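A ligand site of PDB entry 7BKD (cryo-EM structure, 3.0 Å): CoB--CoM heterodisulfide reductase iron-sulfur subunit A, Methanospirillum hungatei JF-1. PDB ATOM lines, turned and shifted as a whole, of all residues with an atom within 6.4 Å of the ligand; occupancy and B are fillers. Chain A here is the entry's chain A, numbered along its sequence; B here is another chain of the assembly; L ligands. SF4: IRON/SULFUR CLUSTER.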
ATOM      1  N   VAL A 400      26.430   1.761   8.731  1.00  0.00           N
ATOM      2  CA  VAL A 400      25.259   2.164   9.499  1.00  0.00           C
ATOM      3  C   VAL A 400      24.909   3.583   9.083  1.00  0.00           C
ATOM      4  O   VAL A 400      25.614   4.536   9.423  1.00  0.00           O
ATOM      5  CB  VAL A 400      25.507   2.051  11.005  1.00  0.00           C
ATOM      6  CG1 VAL A 400      24.252   2.421  11.781  1.00  0.00           C
ATOM      7  CG2 VAL A 400      25.968   0.659  11.363  1.00  0.00           C
ATOM      8  N   LEU A 401      23.839   3.739   8.324  1.00  0.00           N
ATOM      9  CA  LEU A 401      23.451   5.067   7.829  1.00  0.00           C
ATOM     10  C   LEU A 401      22.515   5.714   8.849  1.00  0.00           C
ATOM     11  O   LEU A 401      21.928   4.971   9.630  1.00  0.00           O
ATOM     12  CB  LEU A 401      22.759   4.906   6.477  1.00  0.00           C
ATOM     13  CG  LEU A 401      23.678   4.865   5.249  1.00  0.00           C
ATOM     14  CD1 LEU A 401      24.456   3.563   5.177  1.00  0.00           C
ATOM     15  CD2 LEU A 401      22.869   5.063   3.977  1.00  0.00           C
ATOM     16  N   CYS A 402      22.496   7.039   8.915  1.00  0.00           N
ATOM     17  CA  CYS A 402      21.552   7.786   9.795  1.00  0.00           C
ATOM     18  C   CYS A 402      22.095   7.723  11.230  1.00  0.00           C
ATOM     19  O   CYS A 402      21.320   7.977  12.129  1.00  0.00           O
ATOM     20  CB  CYS A 402      20.114   7.330   9.616  1.00  0.00           C
ATOM     21  SG  CYS A 402      19.340   7.802   8.051  1.00  0.00           S
ATOM     22  N   ALA A 403      23.381   7.404  11.403  1.00  0.00           N
ATOM     23  CA  ALA A 403      23.944   7.187  12.739  1.00  0.00           C
ATOM     24  C   ALA A 403      23.914   8.500  13.500  1.00  0.00           C
ATOM     25  O   ALA A 403      24.721   9.394  13.265  1.00  0.00           O
ATOM     26  CB  ALA A 403      25.373   6.645  12.632  1.00  0.00           C
ATOM     27  N   SER A 405      21.211  10.521  13.439  1.00  0.00           N
ATOM     28  CA  SER A 405      20.477  11.519  12.617  1.00  0.00           C
ATOM     29  C   SER A 405      18.971  11.240  12.570  1.00  0.00           C
ATOM     30  O   SER A 405      18.586  10.112  12.885  1.00  0.00           O
ATOM     31  CB  SER A 405      21.088  11.608  11.248  1.00  0.00           C
ATOM     32  OG  SER A 405      22.485  11.359  11.294  1.00  0.00           O
ATOM     33  N   ARG A 406      18.156  12.227  12.188  1.00  0.00           N
ATOM     34  CA  ARG A 406      16.685  12.073  12.154  1.00  0.00           C
ATOM     35  C   ARG A 406      16.310  11.495  13.527  1.00  0.00           C
ATOM     36  O   ARG A 406      15.339  10.748  13.588  1.00  0.00           O
ATOM     37  CB  ARG A 406      16.315  11.251  10.922  1.00  0.00           C
ATOM     38  CG  ARG A 406      17.081  11.669   9.668  1.00  0.00           C
ATOM     39  CD  ARG A 406      16.860  10.759   8.479  1.00  0.00           C
ATOM     40  NE  ARG A 406      15.438  10.531   8.259  1.00  0.00           N
ATOM     41  CZ  ARG A 406      14.939   9.561   7.516  1.00  0.00           C
ATOM     42  NH1 ARG A 406      15.760   8.715   6.908  1.00  0.00           N
ATOM     43  NH2 ARG A 406      13.635   9.448   7.369  1.00  0.00           N
ATOM     44  N   TYR A 415      17.882  16.311  12.375  1.00  0.00           N
ATOM     45  CA  TYR A 415      17.924  16.669  10.961  1.00  0.00           C
ATOM     46  C   TYR A 415      18.692  15.620  10.171  1.00  0.00           C
ATOM     47  O   TYR A 415      19.280  14.687  10.722  1.00  0.00           O
ATOM     48  CB  TYR A 415      18.554  18.052  10.766  1.00  0.00           C
ATOM     49  CG  TYR A 415      19.910  18.236  11.419  1.00  0.00           C
ATOM     50  CD1 TYR A 415      20.030  18.944  12.606  1.00  0.00           C
ATOM     51  CD2 TYR A 415      21.058  17.717  10.841  1.00  0.00           C
ATOM     52  CE1 TYR A 415      21.258  19.117  13.204  1.00  0.00           C
ATOM     53  CE2 TYR A 415      22.291  17.895  11.423  1.00  0.00           C
ATOM     54  CZ  TYR A 415      22.389  18.592  12.612  1.00  0.00           C
ATOM     55  OH  TYR A 415      23.611  18.767  13.203  1.00  0.00           O
ATOM     56  N   CYS A 416      18.655  15.765   8.854  1.00  0.00           N
ATOM     57  CA  CYS A 416      19.384  14.844   7.966  1.00  0.00           C
ATOM     58  C   CYS A 416      20.711  15.514   7.655  1.00  0.00           C
ATOM     59  O   CYS A 416      20.721  16.724   7.517  1.00  0.00           O
ATOM     60  CB  CYS A 416      18.540  14.605   6.707  1.00  0.00           C
ATOM     61  SG  CYS A 416      19.410  13.825   5.334  1.00  0.00           S
ATOM     62  N   SER A 417      21.770  14.734   7.534  1.00  0.00           N
ATOM     63  CA  SER A 417      23.108  15.313   7.260  1.00  0.00           C
ATOM     64  C   SER A 417      23.368  15.452   5.754  1.00  0.00           C
ATOM     65  O   SER A 417      24.511  15.770   5.399  1.00  0.00           O
ATOM     66  CB  SER A 417      24.209  14.706   8.079  1.00  0.00           C
ATOM     67  OG  SER A 417      24.167  15.210   9.404  1.00  0.00           O
ATOM     68  N   ARG A 418      22.394  15.118   4.905  1.00  0.00           N
ATOM     69  CA  ARG A 418      22.454  15.405   3.435  1.00  0.00           C
ATOM     70  C   ARG A 418      23.412  14.533   2.609  1.00  0.00           C
ATOM     71  O   ARG A 418      22.982  14.106   1.549  1.00  0.00           O
ATOM     72  CB  ARG A 418      22.622  16.909   3.181  1.00  0.00           C
ATOM     73  CG  ARG A 418      22.195  17.381   1.805  1.00  0.00           C
ATOM     74  CD  ARG A 418      21.902  18.863   1.825  1.00  0.00           C
ATOM     75  NE  ARG A 418      21.893  19.462   0.505  1.00  0.00           N
ATOM     76  CZ  ARG A 418      21.223  20.574   0.201  1.00  0.00           C
ATOM     77  NH1 ARG A 418      20.522  21.186   1.143  1.00  0.00           N
ATOM     78  NH2 ARG A 418      21.258  21.054  -1.024  1.00  0.00           N
ATOM     79  N   PHE A 419      24.646  14.332   3.044  1.00  0.00           N
ATOM     80  CA  PHE A 419      25.638  13.624   2.199  1.00  0.00           C
ATOM     81  C   PHE A 419      26.040  12.231   2.696  1.00  0.00           C
ATOM     82  O   PHE A 419      26.770  11.560   1.965  1.00  0.00           O
ATOM     83  CB  PHE A 419      26.870  14.519   2.000  1.00  0.00           C
ATOM     84  CG  PHE A 419      27.382  15.256   3.216  1.00  0.00           C
ATOM     85  CD1 PHE A 419      27.293  16.633   3.284  1.00  0.00           C
ATOM     86  CD2 PHE A 419      27.967  14.577   4.265  1.00  0.00           C
ATOM     87  CE1 PHE A 419      27.767  17.318   4.390  1.00  0.00           C
ATOM     88  CE2 PHE A 419      28.442  15.262   5.371  1.00  0.00           C
ATOM     89  CZ  PHE A 419      28.352  16.635   5.425  1.00  0.00           C
ATOM     90  N   CYS A 420      25.563  11.804   3.872  1.00  0.00           N
ATOM     91  CA  CYS A 420      25.992  10.499   4.456  1.00  0.00           C
ATOM     92  C   CYS A 420      25.530   9.314   3.598  1.00  0.00           C
ATOM     93  O   CYS A 420      26.274   8.340   3.532  1.00  0.00           O
ATOM     94  CB  CYS A 420      25.689  10.378   5.935  1.00  0.00           C
ATOM     95  SG  CYS A 420      24.765  11.781   6.602  1.00  0.00           S
ATOM     96  N   CYS A 421      24.376   9.415   2.947  1.00  0.00           N
ATOM     97  CA  CYS A 421      23.930   8.334   2.019  1.00  0.00           C
ATOM     98  C   CYS A 421      24.934   8.224   0.851  1.00  0.00           C
ATOM     99  O   CYS A 421      25.346   7.094   0.577  1.00  0.00           O
ATOM    100  CB  CYS A 421      22.535   8.608   1.456  1.00  0.00           C
ATOM    101  SG  CYS A 421      21.156   8.168   2.534  1.00  0.00           S
ATOM    102  N   MET A 422      25.378   9.334   0.264  1.00  0.00           N
ATOM    103  CA  MET A 422      26.214   9.372  -0.932  1.00  0.00           C
ATOM    104  C   MET A 422      27.635   8.902  -0.627  1.00  0.00           C
ATOM    105  O   MET A 422      28.195   8.078  -1.371  1.00  0.00           O
ATOM    106  CB  MET A 422      26.221  10.779  -1.520  1.00  0.00           C
ATOM    107  CG  MET A 422      24.882  11.235  -2.076  1.00  0.00           C
ATOM    108  SD  MET A 422      24.014  10.046  -3.130  1.00  0.00           S
ATOM    109  CE  MET A 422      25.280   9.637  -4.326  1.00  0.00           C
ATOM    110  N   TYR A 423      28.240   9.389   0.461  1.00  0.00           N
ATOM    111  CA  TYR A 423      29.592   8.902   0.727  1.00  0.00           C
ATOM    112  C   TYR A 423      29.596   7.494   1.293  1.00  0.00           C
ATOM    113  O   TYR A 423      30.611   6.809   1.163  1.00  0.00           O
ATOM    114  CB  TYR A 423      30.399   9.854   1.635  1.00  0.00           C
ATOM    115  CG  TYR A 423      29.972  10.019   3.080  1.00  0.00           C
ATOM    116  CD1 TYR A 423      29.475  11.230   3.532  1.00  0.00           C
ATOM    117  CD2 TYR A 423      30.098   8.981   3.992  1.00  0.00           C
ATOM    118  CE1 TYR A 423      29.103  11.393   4.854  1.00  0.00           C
ATOM    119  CE2 TYR A 423      29.704   9.130   5.303  1.00  0.00           C
ATOM    120  CZ  TYR A 423      29.218  10.341   5.732  1.00  0.00           C
ATOM    121  OH  TYR A 423      28.846  10.500   7.041  1.00  0.00           O
ATOM    122  N   SER A 424      28.498   7.032   1.880  1.00  0.00           N
ATOM    123  CA  SER A 424      28.405   5.613   2.223  1.00  0.00           C
ATOM    124  C   SER A 424      28.404   4.750   0.972  1.00  0.00           C
ATOM    125  O   SER A 424      29.058   3.703   0.925  1.00  0.00           O
ATOM    126  CB  SER A 424      27.147   5.351   3.060  1.00  0.00           C
ATOM    127  OG  SER A 424      27.239   6.008   4.311  1.00  0.00           O
ATOM    128  N   MET A 445      17.869   3.519   5.816  1.00  0.00           N
ATOM    129  CA  MET A 445      16.486   3.810   6.261  1.00  0.00           C
ATOM    130  C   MET A 445      16.088   5.033   5.464  1.00  0.00           C
ATOM    131  O   MET A 445      16.175   6.132   6.060  1.00  0.00           O
ATOM    132  CB  MET A 445      16.532   4.186   7.749  1.00  0.00           C
ATOM    133  CG  MET A 445      15.212   4.580   8.373  1.00  0.00           C
ATOM    134  SD  MET A 445      15.519   5.170  10.048  1.00  0.00           S
ATOM    135  CE  MET A 445      16.379   6.715   9.754  1.00  0.00           C
ATOM    136  N   ASP A 446      15.848   4.899   4.172  1.00  0.00           N
ATOM    137  CA  ASP A 446      15.594   6.058   3.260  1.00  0.00           C
ATOM    138  C   ASP A 446      16.871   6.490   2.534  1.00  0.00           C
ATOM    139  O   ASP A 446      17.457   7.492   2.942  1.00  0.00           O
ATOM    140  CB  ASP A 446      14.739   7.215   3.805  1.00  0.00           C
ATOM    141  CG  ASP A 446      13.284   6.865   4.066  1.00  0.00           C
ATOM    142  OD1 ASP A 446      12.451   7.178   3.203  1.00  0.00           O
ATOM    143  OD2 ASP A 446      13.004   6.301   5.145  1.00  0.00           O
ATOM    144  N   ILE A 447      17.289   5.743   1.531  1.00  0.00           N
ATOM    145  CA  ILE A 447      18.401   6.114   0.652  1.00  0.00           C
ATOM    146  C   ILE A 447      18.089   7.432  -0.037  1.00  0.00           C
ATOM    147  O   ILE A 447      17.028   7.593  -0.659  1.00  0.00           O
ATOM    148  CB  ILE A 447      18.675   5.003  -0.392  1.00  0.00           C
ATOM    149  CG1 ILE A 447      19.407   3.821   0.249  1.00  0.00           C
ATOM    150  CG2 ILE A 447      19.482   5.551  -1.547  1.00  0.00           C
ATOM    151  CD1 ILE A 447      20.815   4.120   0.678  1.00  0.00           C
ATOM    152  N   ARG A 448      19.002   8.407   0.116  1.00  0.00           N
ATOM    153  CA  ARG A 448      18.735   9.810  -0.318  1.00  0.00           C
ATOM    154  C   ARG A 448      19.738  10.279  -1.388  1.00  0.00           C
ATOM    155  O   ARG A 448      20.697  10.974  -1.021  1.00  0.00           O
ATOM    156  CB  ARG A 448      18.681  10.691   0.929  1.00  0.00           C
ATOM    157  CG  ARG A 448      17.383  10.581   1.714  1.00  0.00           C
ATOM    158  CD  ARG A 448      17.171  11.606   2.793  1.00  0.00           C
ATOM    159  NE  ARG A 448      15.822  11.475   3.329  1.00  0.00           N
ATOM    160  CZ  ARG A 448      15.408  11.954   4.492  1.00  0.00           C
ATOM    161  NH1 ARG A 448      14.159  11.774   4.872  1.00  0.00           N
ATOM    162  NH2 ARG A 448      16.248  12.606   5.271  1.00  0.00           N
ATOM    163  N   PHE A 450      19.654  12.567  -4.210  1.00  0.00           N
ATOM    164  CA  PHE A 450      18.806  13.602  -4.764  1.00  0.00           C
ATOM    165  C   PHE A 450      19.496  14.469  -5.808  1.00  0.00           C
ATOM    166  O   PHE A 450      18.814  15.068  -6.640  1.00  0.00           O
ATOM    167  CB  PHE A 450      18.299  14.512  -3.641  1.00  0.00           C
ATOM    168  CG  PHE A 450      19.401  15.119  -2.822  1.00  0.00           C
ATOM    169  CD1 PHE A 450      19.944  16.347  -3.176  1.00  0.00           C
ATOM    170  CD2 PHE A 450      19.910  14.461  -1.721  1.00  0.00           C
ATOM    171  CE1 PHE A 450      20.968  16.896  -2.438  1.00  0.00           C
ATOM    172  CE2 PHE A 450      20.930  15.002  -0.980  1.00  0.00           C
ATOM    173  CZ  PHE A 450      21.455  16.229  -1.334  1.00  0.00           C
ATOM    174  N   ALA A 508      28.025   6.151   9.680  1.00  0.00           N
ATOM    175  CA  ALA A 508      27.823   7.408   8.954  1.00  0.00           C
ATOM    176  C   ALA A 508      27.255   8.426   9.941  1.00  0.00           C
ATOM    177  O   ALA A 508      26.044   8.697   9.984  1.00  0.00           O
ATOM    178  CB  ALA A 508      26.930   7.210   7.743  1.00  0.00           C
ATOM    179  N   ALA A 509      28.135   8.993  10.748  1.00  0.00           N
ATOM    180  CA  ALA A 509      27.729   9.872  11.835  1.00  0.00           C
ATOM    181  C   ALA A 509      27.211  11.206  11.302  1.00  0.00           C
ATOM    182  O   ALA A 509      27.555  11.647  10.210  1.00  0.00           O
ATOM    183  CB  ALA A 509      28.890  10.113  12.788  1.00  0.00           C
ATOM    184  N   SER B 449      13.790  14.308   2.382  1.00  0.00           N
ATOM    185  CA  SER B 449      13.803  15.625   3.019  1.00  0.00           C
ATOM    186  C   SER B 449      15.213  15.833   3.557  1.00  0.00           C
ATOM    187  O   SER B 449      15.498  15.556   4.725  1.00  0.00           O
ATOM    188  CB  SER B 449      12.741  15.728   4.115  1.00  0.00           C
ATOM    189  OG  SER B 449      12.858  14.662   5.041  1.00  0.00           O
ATOM    190  N   PHE B 450      16.103  16.325   2.700  1.00  0.00           N
ATOM    191  CA  PHE B 450      17.533  16.321   2.956  1.00  0.00           C
ATOM    192  C   PHE B 450      18.072  17.668   3.410  1.00  0.00           C
ATOM    193  O   PHE B 450      19.130  17.702   4.049  1.00  0.00           O
ATOM    194  CB  PHE B 450      18.286  15.906   1.689  1.00  0.00           C
ATOM    195  CG  PHE B 450      17.857  16.665   0.467  1.00  0.00           C
ATOM    196  CD1 PHE B 450      18.492  17.842   0.119  1.00  0.00           C
ATOM    197  CD2 PHE B 450      16.809  16.214  -0.310  1.00  0.00           C
ATOM    198  CE1 PHE B 450      18.093  18.550  -0.996  1.00  0.00           C
ATOM    199  CE2 PHE B 450      16.406  16.914  -1.422  1.00  0.00           C
ATOM    200  CZ  PHE B 450      17.053  18.084  -1.769  1.00  0.00           C
ATOM    201  N   GLU B 455      13.587  17.854   7.196  1.00  0.00           N
ATOM    202  CA  GLU B 455      13.175  16.708   7.996  1.00  0.00           C
ATOM    203  C   GLU B 455      12.149  17.121   9.052  1.00  0.00           C
ATOM    204  O   GLU B 455      11.201  16.366   9.326  1.00  0.00           O
ATOM    205  CB  GLU B 455      14.392  16.051   8.646  1.00  0.00           C
ATOM    206  CG  GLU B 455      14.077  14.819   9.467  1.00  0.00           C
ATOM    207  CD  GLU B 455      14.013  13.554   8.635  1.00  0.00           C
ATOM    208  OE1 GLU B 455      13.511  12.525   9.130  1.00  0.00           O
ATOM    209  OE2 GLU B 455      14.473  13.591   7.468  1.00  0.00           O
HETATM  210 FE1  SF4 L   1      22.757  10.844   6.258  1.00  0.00          FE
HETATM  211 FE2  SF4 L   1      20.566   9.353   6.917  1.00  0.00          FE
HETATM  212 FE3  SF4 L   1      21.294   9.574   4.299  1.00  0.00          FE
HETATM  213 FE4  SF4 L   1      20.270  11.764   5.631  1.00  0.00          FE
HETATM  214  S1  SF4 L   1      19.197   9.797   5.148  1.00  0.00           S
HETATM  215  S2  SF4 L   1      22.080  11.718   4.258  1.00  0.00           S
HETATM  216  S3  SF4 L   1      21.103  11.422   7.710  1.00  0.00           S
HETATM  217  S4  SF4 L   1      22.495   8.601   5.974  1.00  0.00           S
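A sulfur (S1) of the ligand sits close to the backbone carbonyl oxygen (O) of Asp 446 (3.6 Å). Residues that only touch the ligand: Ser 405 (3.5 Å), Arg 448 (3.6 Å), Leu 401 (3.7 Å) and Phe 419 (3.9 Å).
The backbone NH (N) of Cys 420 sits close to a sulfur (S2) of the ligand, at 3.5 Å. An iron atom (FE1) of the ligand is bound by the side-chain sulfur (SG) of Cys 420. An iron atom (FE4) of the ligand is bound by the side-chain sulfur of Cys 416 (2.3 Å). A sulfur (S2) of the ligand sits close to the backbone NH of Cys 421. SG of Cys 421 is bound to FE3 of the ligand, at 2.3 Å. S4 of the ligand sits close to N of Cys 402. SG of Cys 402 binds FE2 of the ligand (2.3 Å). N of Ser 417 sits close to S3 of the ligand, 3.4 Å away. N of Arg 418 lies close to S2 of the ligand.
O of Cys 420 lies within hydrogen-bond range of OG of Ser 424, at 2.6 Å. The side-chain sulfur (SG) of Cys 416 lies close to the backbone NH (N) of Arg 418 (3.3 Å). NH2 of Arg 448 sits close to SG of Cys 416 (3.4 Å). The backbone NH of Arg 448 lies close to the side-chain sulfur of Cys 421, at 3.2 Å. The side-chain sulfur of Cys 421 lies close to the backbone carbonyl oxygen of Asp 446, 3.8 Å away. The backbone carbonyl oxygen of Ser 449 of chain B lies within hydrogen-bond range of the guanidinium group of Arg 448 (3.1 Å). The guanidinium group (NH2) of Arg 448 lies within salt-bridge range of the side-chain carboxylate (OE2) of Glu 455 of chain B (3.0 Å). The side-chain carboxylate of Asp 446 lies within salt-bridge range of the guanidinium group of Arg 406, at 3.9 Å.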
